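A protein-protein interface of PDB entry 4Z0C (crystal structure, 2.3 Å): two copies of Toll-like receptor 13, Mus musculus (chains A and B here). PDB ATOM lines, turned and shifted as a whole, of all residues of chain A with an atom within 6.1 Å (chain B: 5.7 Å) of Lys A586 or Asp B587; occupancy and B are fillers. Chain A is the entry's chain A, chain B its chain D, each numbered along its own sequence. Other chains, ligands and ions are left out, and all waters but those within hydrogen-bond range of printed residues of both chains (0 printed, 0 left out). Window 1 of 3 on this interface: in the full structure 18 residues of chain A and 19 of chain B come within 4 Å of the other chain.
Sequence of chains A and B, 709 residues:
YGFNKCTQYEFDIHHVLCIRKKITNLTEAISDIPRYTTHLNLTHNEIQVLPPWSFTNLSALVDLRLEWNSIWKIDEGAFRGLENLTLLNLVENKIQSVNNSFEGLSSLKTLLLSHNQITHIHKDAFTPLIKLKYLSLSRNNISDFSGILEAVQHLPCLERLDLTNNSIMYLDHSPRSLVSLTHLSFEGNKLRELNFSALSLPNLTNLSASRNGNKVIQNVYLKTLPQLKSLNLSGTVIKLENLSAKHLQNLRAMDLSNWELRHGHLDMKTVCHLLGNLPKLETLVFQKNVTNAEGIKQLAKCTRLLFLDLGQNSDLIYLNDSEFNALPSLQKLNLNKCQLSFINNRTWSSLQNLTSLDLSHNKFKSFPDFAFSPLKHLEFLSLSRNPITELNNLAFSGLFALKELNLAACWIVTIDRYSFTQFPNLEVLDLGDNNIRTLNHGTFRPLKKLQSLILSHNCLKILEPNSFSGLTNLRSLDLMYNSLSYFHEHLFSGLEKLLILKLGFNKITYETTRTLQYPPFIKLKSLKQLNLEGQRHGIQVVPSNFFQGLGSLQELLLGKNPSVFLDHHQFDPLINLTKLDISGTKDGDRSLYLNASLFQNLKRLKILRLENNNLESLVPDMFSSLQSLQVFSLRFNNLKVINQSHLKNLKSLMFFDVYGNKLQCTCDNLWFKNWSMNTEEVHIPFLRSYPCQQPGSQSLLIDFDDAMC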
ATOM      1  N   ASN A 561      -6.984 -18.154 -20.562  1.00  0.00           N
ATOM      2  CA  ASN A 561      -7.836 -19.045 -19.766  1.00  0.00           C
ATOM      3  C   ASN A 561      -8.527 -20.096 -20.656  1.00  0.00           C
ATOM      4  O   ASN A 561      -9.049 -19.766 -21.720  1.00  0.00           O
ATOM      5  CB  ASN A 561      -8.894 -18.249 -18.997  1.00  0.00           C
ATOM      6  CG  ASN A 561      -8.352 -17.608 -17.731  1.00  0.00           C
ATOM      7  OD1 ASN A 561      -8.161 -18.276 -16.715  1.00  0.00           O
ATOM      8  ND2 ASN A 561      -8.117 -16.304 -17.781  1.00  0.00           N
ATOM      9  N   PRO A 562      -8.494 -21.371 -20.241  1.00  0.00           N
ATOM     10  CA  PRO A 562      -9.191 -22.462 -20.930  1.00  0.00           C
ATOM     11  C   PRO A 562     -10.677 -22.168 -21.107  1.00  0.00           C
ATOM     12  O   PRO A 562     -11.256 -22.615 -22.091  1.00  0.00           O
ATOM     13  CB  PRO A 562      -8.992 -23.649 -19.990  1.00  0.00           C
ATOM     14  CG  PRO A 562      -7.678 -23.382 -19.347  1.00  0.00           C
ATOM     15  CD  PRO A 562      -7.594 -21.874 -19.189  1.00  0.00           C
ATOM     16  N   SER A 583      -8.161 -13.047 -24.786  1.00  0.00           N
ATOM     17  CA  SER A 583      -7.694 -13.813 -25.927  1.00  0.00           C
ATOM     18  C   SER A 583      -7.249 -15.193 -25.499  1.00  0.00           C
ATOM     19  O   SER A 583      -6.914 -15.402 -24.343  1.00  0.00           O
ATOM     20  CB  SER A 583      -6.531 -13.084 -26.604  1.00  0.00           C
ATOM     21  OG  SER A 583      -6.909 -11.753 -26.912  1.00  0.00           O
ATOM     22  N   GLY A 584      -7.259 -16.133 -26.438  1.00  0.00           N
ATOM     23  CA  GLY A 584      -6.625 -17.419 -26.235  1.00  0.00           C
ATOM     24  C   GLY A 584      -7.435 -18.486 -25.507  1.00  0.00           C
ATOM     25  O   GLY A 584      -6.843 -19.412 -24.985  1.00  0.00           O
ATOM     26  N   THR A 585      -8.764 -18.374 -25.457  1.00  0.00           N
ATOM     27  CA  THR A 585      -9.575 -19.471 -24.932  1.00  0.00           C
ATOM     28  C   THR A 585      -9.668 -20.604 -25.953  1.00  0.00           C
ATOM     29  O   THR A 585      -9.863 -21.754 -25.588  1.00  0.00           O
ATOM     30  CB  THR A 585     -10.979 -19.021 -24.474  1.00  0.00           C
ATOM     31  OG1 THR A 585     -11.853 -18.846 -25.611  1.00  0.00           O
ATOM     32  CG2 THR A 585     -10.886 -17.737 -23.655  1.00  0.00           C
ATOM     33  N   LYS A 586      -9.582 -20.253 -27.233  1.00  0.00           N
ATOM     34  CA  LYS A 586      -9.315 -21.214 -28.305  1.00  0.00           C
ATOM     35  C   LYS A 586     -10.448 -22.115 -28.799  1.00  0.00           C
ATOM     36  O   LYS A 586     -10.252 -22.818 -29.784  1.00  0.00           O
ATOM     37  CB  LYS A 586      -8.085 -22.075 -27.992  1.00  0.00           C
ATOM     38  CG  LYS A 586      -6.761 -21.328 -27.965  1.00  0.00           C
ATOM     39  CD  LYS A 586      -5.598 -22.300 -28.155  1.00  0.00           C
ATOM     40  CE  LYS A 586      -4.245 -21.702 -27.739  1.00  0.00           C
ATOM     41  NZ  LYS A 586      -3.998 -21.770 -26.258  1.00  0.00           N
ATOM     42  N   ASP A 587     -11.617 -22.133 -28.166  1.00  0.00           N
ATOM     43  CA  ASP A 587     -12.760 -22.715 -28.891  1.00  0.00           C
ATOM     44  C   ASP A 587     -14.106 -22.135 -28.500  1.00  0.00           C
ATOM     45  O   ASP A 587     -14.891 -22.747 -27.766  1.00  0.00           O
ATOM     46  CB  ASP A 587     -12.778 -24.259 -28.934  1.00  0.00           C
ATOM     47  CG  ASP A 587     -12.820 -24.879 -27.582  1.00  0.00           C
ATOM     48  OD1 ASP A 587     -12.569 -24.148 -26.607  1.00  0.00           O
ATOM     49  OD2 ASP A 587     -13.067 -26.103 -27.497  1.00  0.00           O
ATOM     50  N   GLY A 588     -14.341 -20.953 -29.064  1.00  0.00           N
ATOM     51  CA  GLY A 588     -15.508 -20.118 -28.856  1.00  0.00           C
ATOM     52  C   GLY A 588     -16.607 -20.470 -27.878  1.00  0.00           C
ATOM     53  O   GLY A 588     -16.502 -20.186 -26.680  1.00  0.00           O
ATOM     54  N   SER A 591     -15.703 -22.272 -24.751  1.00  0.00           N
ATOM     55  CA  SER A 591     -14.715 -21.673 -23.848  1.00  0.00           C
ATOM     56  C   SER A 591     -14.966 -20.217 -23.488  1.00  0.00           C
ATOM     57  O   SER A 591     -14.304 -19.676 -22.593  1.00  0.00           O
ATOM     58  CB  SER A 591     -13.302 -21.787 -24.435  1.00  0.00           C
ATOM     59  OG  SER A 591     -13.187 -21.126 -25.677  1.00  0.00           O
ATOM     60  N   GLU A 611      -8.657 -12.209 -29.318  1.00  0.00           N
ATOM     61  CA  GLU A 611      -7.924 -13.007 -30.315  1.00  0.00           C
ATOM     62  C   GLU A 611      -7.834 -14.491 -29.984  1.00  0.00           C
ATOM     63  O   GLU A 611      -7.930 -14.883 -28.828  1.00  0.00           O
ATOM     64  CB  GLU A 611      -6.486 -12.459 -30.492  1.00  0.00           C
ATOM     65  CG  GLU A 611      -6.370 -10.931 -30.390  1.00  0.00           C
ATOM     66  CD  GLU A 611      -4.935 -10.379 -30.542  1.00  0.00           C
ATOM     67  OE1 GLU A 611      -3.947 -11.157 -30.549  1.00  0.00           O
ATOM     68  OE2 GLU A 611      -4.800  -9.140 -30.599  1.00  0.00           O
ATOM     69  N   ASN A 612      -7.614 -15.308 -31.006  1.00  0.00           N
ATOM     70  CA  ASN A 612      -7.371 -16.731 -30.809  1.00  0.00           C
ATOM     71  C   ASN A 612      -8.453 -17.380 -29.954  1.00  0.00           C
ATOM     72  O   ASN A 612      -8.169 -18.151 -29.040  1.00  0.00           O
ATOM     73  CB  ASN A 612      -6.002 -16.969 -30.189  1.00  0.00           C
ATOM     74  CG  ASN A 612      -5.206 -18.021 -30.937  1.00  0.00           C
ATOM     75  OD1 ASN A 612      -5.514 -19.213 -30.887  1.00  0.00           O
ATOM     76  ND2 ASN A 612      -4.169 -17.580 -31.644  1.00  0.00           N
ATOM     77  N   ASN A 613      -9.703 -17.036 -30.238  1.00  0.00           N
ATOM     78  CA  ASN A 613     -10.811 -17.617 -29.506  1.00  0.00           C
ATOM     79  C   ASN A 613     -11.637 -18.491 -30.419  1.00  0.00           C
ATOM     80  O   ASN A 613     -12.665 -19.013 -29.998  1.00  0.00           O
ATOM     81  CB  ASN A 613     -11.682 -16.533 -28.911  1.00  0.00           C
ATOM     82  CG  ASN A 613     -11.124 -15.995 -27.635  1.00  0.00           C
ATOM     83  OD1 ASN A 613     -10.756 -16.757 -26.756  1.00  0.00           O
ATOM     84  ND2 ASN A 613     -11.030 -14.677 -27.530  1.00  0.00           N
ATOM     85  N   ASN A 614     -11.190 -18.646 -31.666  1.00  0.00           N
ATOM     86  CA  ASN A 614     -11.949 -19.414 -32.652  1.00  0.00           C
ATOM     87  C   ASN A 614     -13.426 -19.040 -32.762  1.00  0.00           C
ATOM     88  O   ASN A 614     -14.272 -19.902 -32.981  1.00  0.00           O
ATOM     89  CB  ASN A 614     -11.792 -20.914 -32.391  1.00  0.00           C
ATOM     90  CG  ASN A 614     -10.632 -21.530 -33.154  1.00  0.00           C
ATOM     91  OD1 ASN A 614     -10.767 -22.612 -33.720  1.00  0.00           O
ATOM     92  ND2 ASN A 614      -9.502 -20.834 -33.202  1.00  0.00           N
ATOM     93  N   PRO B 562      -0.613 -27.632 -26.059  1.00  0.00           N
ATOM     94  CA  PRO B 562      -0.929 -26.447 -26.871  1.00  0.00           C
ATOM     95  C   PRO B 562      -0.517 -26.617 -28.342  1.00  0.00           C
ATOM     96  O   PRO B 562      -1.197 -26.123 -29.237  1.00  0.00           O
ATOM     97  CB  PRO B 562      -0.119 -25.350 -26.198  1.00  0.00           C
ATOM     98  CG  PRO B 562      -0.085 -25.760 -24.758  1.00  0.00           C
ATOM     99  CD  PRO B 562      -0.022 -27.270 -24.760  1.00  0.00           C
ATOM    100  N   THR B 585      -5.481 -29.992 -28.489  1.00  0.00           N
ATOM    101  CA  THR B 585      -4.576 -28.923 -28.944  1.00  0.00           C
ATOM    102  C   THR B 585      -5.342 -27.643 -29.249  1.00  0.00           C
ATOM    103  O   THR B 585      -4.797 -26.563 -29.110  1.00  0.00           O
ATOM    104  CB  THR B 585      -3.735 -29.300 -30.183  1.00  0.00           C
ATOM    105  OG1 THR B 585      -4.531 -29.191 -31.375  1.00  0.00           O
ATOM    106  CG2 THR B 585      -3.163 -30.701 -30.041  1.00  0.00           C
ATOM    107  N   LYS B 586      -6.598 -27.789 -29.672  1.00  0.00           N
ATOM    108  CA  LYS B 586      -7.575 -26.686 -29.733  1.00  0.00           C
ATOM    109  C   LYS B 586      -7.563 -25.683 -30.911  1.00  0.00           C
ATOM    110  O   LYS B 586      -8.407 -24.791 -30.927  1.00  0.00           O
ATOM    111  CB  LYS B 586      -7.624 -25.894 -28.422  1.00  0.00           C
ATOM    112  CG  LYS B 586      -8.187 -26.634 -27.223  1.00  0.00           C
ATOM    113  CD  LYS B 586      -8.618 -25.614 -26.174  1.00  0.00           C
ATOM    114  CE  LYS B 586      -8.787 -26.224 -24.814  1.00  0.00           C
ATOM    115  NZ  LYS B 586      -7.461 -26.362 -24.160  1.00  0.00           N
ATOM    116  N   ASP B 587      -6.618 -25.772 -31.850  1.00  0.00           N
ATOM    117  CA  ASP B 587      -6.769 -25.040 -33.120  1.00  0.00           C
ATOM    118  C   ASP B 587      -6.057 -25.556 -34.363  1.00  0.00           C
ATOM    119  O   ASP B 587      -5.052 -24.980 -34.800  1.00  0.00           O
ATOM    120  CB  ASP B 587      -6.574 -23.522 -32.983  1.00  0.00           C
ATOM    121  CG  ASP B 587      -5.310 -23.168 -32.295  1.00  0.00           C
ATOM    122  OD1 ASP B 587      -4.796 -24.046 -31.574  1.00  0.00           O
ATOM    123  OD2 ASP B 587      -4.836 -22.027 -32.486  1.00  0.00           O
ATOM    124  N   GLY B 588      -6.694 -26.556 -34.970  1.00  0.00           N
ATOM    125  CA  GLY B 588      -6.217 -27.304 -36.119  1.00  0.00           C
ATOM    126  C   GLY B 588      -4.818 -27.043 -36.607  1.00  0.00           C
ATOM    127  O   GLY B 588      -3.862 -27.548 -36.002  1.00  0.00           O
ATOM    128  N   ASP B 589      -4.700 -26.251 -37.674  1.00  0.00           N
ATOM    129  CA  ASP B 589      -3.432 -26.053 -38.393  1.00  0.00           C
ATOM    130  C   ASP B 589      -2.316 -25.374 -37.600  1.00  0.00           C
ATOM    131  O   ASP B 589      -1.137 -25.674 -37.795  1.00  0.00           O
ATOM    132  CB  ASP B 589      -3.674 -25.313 -39.707  1.00  0.00           C
ATOM    133  CG  ASP B 589      -4.159 -26.238 -40.815  1.00  0.00           C
ATOM    134  OD1 ASP B 589      -3.816 -27.440 -40.772  1.00  0.00           O
ATOM    135  OD2 ASP B 589      -4.887 -25.771 -41.721  1.00  0.00           O
ATOM    136  N   ARG B 590      -2.688 -24.451 -36.720  1.00  0.00           N
ATOM    137  CA  ARG B 590      -1.716 -23.755 -35.884  1.00  0.00           C
ATOM    138  C   ARG B 590      -1.098 -24.629 -34.794  1.00  0.00           C
ATOM    139  O   ARG B 590       0.043 -24.416 -34.389  1.00  0.00           O
ATOM    140  CB  ARG B 590      -2.367 -22.537 -35.228  1.00  0.00           C
ATOM    141  CG  ARG B 590      -2.676 -21.389 -36.193  1.00  0.00           C
ATOM    142  CD  ARG B 590      -3.275 -20.224 -35.439  1.00  0.00           C
ATOM    143  NE  ARG B 590      -4.311 -19.583 -36.225  1.00  0.00           N
ATOM    144  CZ  ARG B 590      -5.611 -19.665 -35.980  1.00  0.00           C
ATOM    145  NH1 ARG B 590      -6.056 -20.369 -34.951  1.00  0.00           N
ATOM    146  NH2 ARG B 590      -6.464 -19.030 -36.774  1.00  0.00           N
ATOM    147  N   SER B 591      -1.873 -25.580 -34.289  1.00  0.00           N
ATOM    148  CA  SER B 591      -1.479 -26.356 -33.120  1.00  0.00           C
ATOM    149  C   SER B 591      -1.199 -27.839 -33.386  1.00  0.00           C
ATOM    150  O   SER B 591      -0.662 -28.534 -32.529  1.00  0.00           O
ATOM    151  CB  SER B 591      -2.546 -26.214 -32.033  1.00  0.00           C
ATOM    152  OG  SER B 591      -3.803 -26.638 -32.511  1.00  0.00           O
ATOM    153  N   LEU B 592      -1.552 -28.327 -34.567  1.00  0.00           N
ATOM    154  CA  LEU B 592      -1.413 -29.746 -34.847  1.00  0.00           C
ATOM    155  C   LEU B 592      -0.959 -29.982 -36.278  1.00  0.00           C
ATOM    156  O   LEU B 592      -1.620 -29.540 -37.210  1.00  0.00           O
ATOM    157  CB  LEU B 592      -2.768 -30.445 -34.640  1.00  0.00           C
ATOM    158  CG  LEU B 592      -2.868 -31.895 -34.165  1.00  0.00           C
ATOM    159  CD1 LEU B 592      -4.125 -32.569 -34.729  1.00  0.00           C
ATOM    160  CD2 LEU B 592      -1.627 -32.697 -34.484  1.00  0.00           C
ATOM    161  N   ASN B 612     -11.276 -32.459 -29.877  1.00  0.00           N
ATOM    162  CA  ASN B 612     -11.075 -31.098 -29.422  1.00  0.00           C
ATOM    163  C   ASN B 612      -9.854 -30.440 -30.033  1.00  0.00           C
ATOM    164  O   ASN B 612      -9.100 -29.770 -29.342  1.00  0.00           O
ATOM    165  CB  ASN B 612     -10.970 -31.040 -27.907  1.00  0.00           C
ATOM    166  CG  ASN B 612     -11.811 -29.941 -27.324  1.00  0.00           C
ATOM    167  OD1 ASN B 612     -11.509 -28.758 -27.489  1.00  0.00           O
ATOM    168  ND2 ASN B 612     -12.871 -30.323 -26.620  1.00  0.00           N
ATOM    169  N   ASN B 613      -9.678 -30.633 -31.333  1.00  0.00           N
ATOM    170  CA  ASN B 613      -8.547 -30.082 -32.036  1.00  0.00           C
ATOM    171  C   ASN B 613      -8.965 -29.003 -33.027  1.00  0.00           C
ATOM    172  O   ASN B 613      -8.137 -28.486 -33.772  1.00  0.00           O
ATOM    173  CB  ASN B 613      -7.795 -31.204 -32.756  1.00  0.00           C
ATOM    174  CG  ASN B 613      -6.889 -31.968 -31.826  1.00  0.00           C
ATOM    175  OD1 ASN B 613      -6.173 -31.367 -31.029  1.00  0.00           O
ATOM    176  ND2 ASN B 613      -6.910 -33.292 -31.920  1.00  0.00           N
ATOM    177  N   ASN B 614     -10.253 -28.670 -33.031  1.00  0.00           N
ATOM    178  CA  ASN B 614     -10.790 -27.693 -33.980  1.00  0.00           C
ATOM    179  C   ASN B 614     -10.376 -27.961 -35.418  1.00  0.00           C
ATOM    180  O   ASN B 614     -10.115 -27.033 -36.167  1.00  0.00           O
ATOM    181  CB  ASN B 614     -10.434 -26.261 -33.561  1.00  0.00           C
ATOM    182  CG  ASN B 614     -11.414 -25.705 -32.547  1.00  0.00           C
ATOM    183  OD1 ASN B 614     -11.050 -25.396 -31.407  1.00  0.00           O
ATOM    184  ND2 ASN B 614     -12.681 -25.608 -32.946  1.00  0.00           N
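Of the 12 printed residues of chain B, 5 touch a printed residue of chain A.
Of the 13 printed residues of chain A, 4 touch a printed residue of chain B.
Among the printed residues, no Asp or Glu carboxylate lies within 4 Å of a Lys or Arg side-chain nitrogen of the other chain.
The backbone NH (N) of Gly A584 sits close to the backbone carbonyl oxygen (O) of Asn A612 (3.4 Å).
The backbone NH (N) of Lys A586 sits at hydrogen-bond distance from the backbone carbonyl oxygen (O) of Asn A612.
N of Asp A587 is in hydrogen-bond range of OG of Ser A591.
N of Lys B586 is in hydrogen-bond range of O of Asn B612.
The backbone carbonyl oxygen (O) of Lys B586 lies close to the side-chain amide oxygen (OD1) of Asn B614 (2.8 Å).
The side-chain carboxylate (OD2) of Asp B587 is in salt-bridge range of the guanidinium group (NH1) of Arg B590 (3.2 Å).
The backbone carbonyl oxygen (O) of Lys A586 lies close to the side-chain amide oxygen (OD1) of Asn B614, 3.1 Å away.
The side-chain carboxylate of Asp A587 lies close to the side-chain amide oxygen of Asn B612, 3.1 Å away.
OD1 of Asn A612 lies close to OD2 of Asp B587 (3.3 Å).
The backbone carbonyl oxygen of Lys A586 lies close to the backbone carbonyl oxygen of Lys B586, 2.9 Å away.
Lys A586 touches its own counterpart, Lys B586.
Lys A586 touches Asp B587, but with the chains exchanged Asp A587 does not touch Lys B586 (4.2 Å).
Lys A586 touches Asn B614, but with the chains exchanged Asn A614 does not touch Lys B586 (4.3 Å).
Asn A614 touches its own counterpart, Asn B614.
Of the 9 pairs that touch across the chains among the printed residues, 6 have their exchanged pair printed and touching as well.
Of chain B, only Lys B586 (2.9 Å), Asp B587 (3.9 Å) and Asn B614 (3.1 Å) come within 4 Å of Lys A586.
Printed residues of chain B within 4 Å of Asn A614: Asp B587 (3.98 Å), Arg B590 (3.9 Å) and Asn B614 (3.4 Å).
Printed residues of chain A within 4 Å of Asp B587: Lys A586, Asn A612 and Asn A614.
Gly B588 touches none of the printed residues of chain A.
Of the printed residues of chain A, Arg B590 touches Asn A614.
Of the printed residues of chain A, Asn B612 touches Asp A587 (3.1 Å).
Printed residues of chain A within 4 Å of Asn B614: Lys A586, Asp A587 and Asn A614.
The nearest printed residue of chain A that does not touch Asp B587 is Asp A587 (7.0 Å).
The nearest printed residue of chain B that does not touch Asn A614 is Lys B586 (4.3 Å).
Among the printed residues, pairs that only touch across the chains: Asp A587 with Asn B614 (3.2 Å), Asn A614 with Asn B614 (3.4 Å), Asn A614 with Arg B590 (3.9 Å), Lys A586 with Asp B587 (3.9 Å) and Asn A614 with Asp B587 (3.98 Å).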
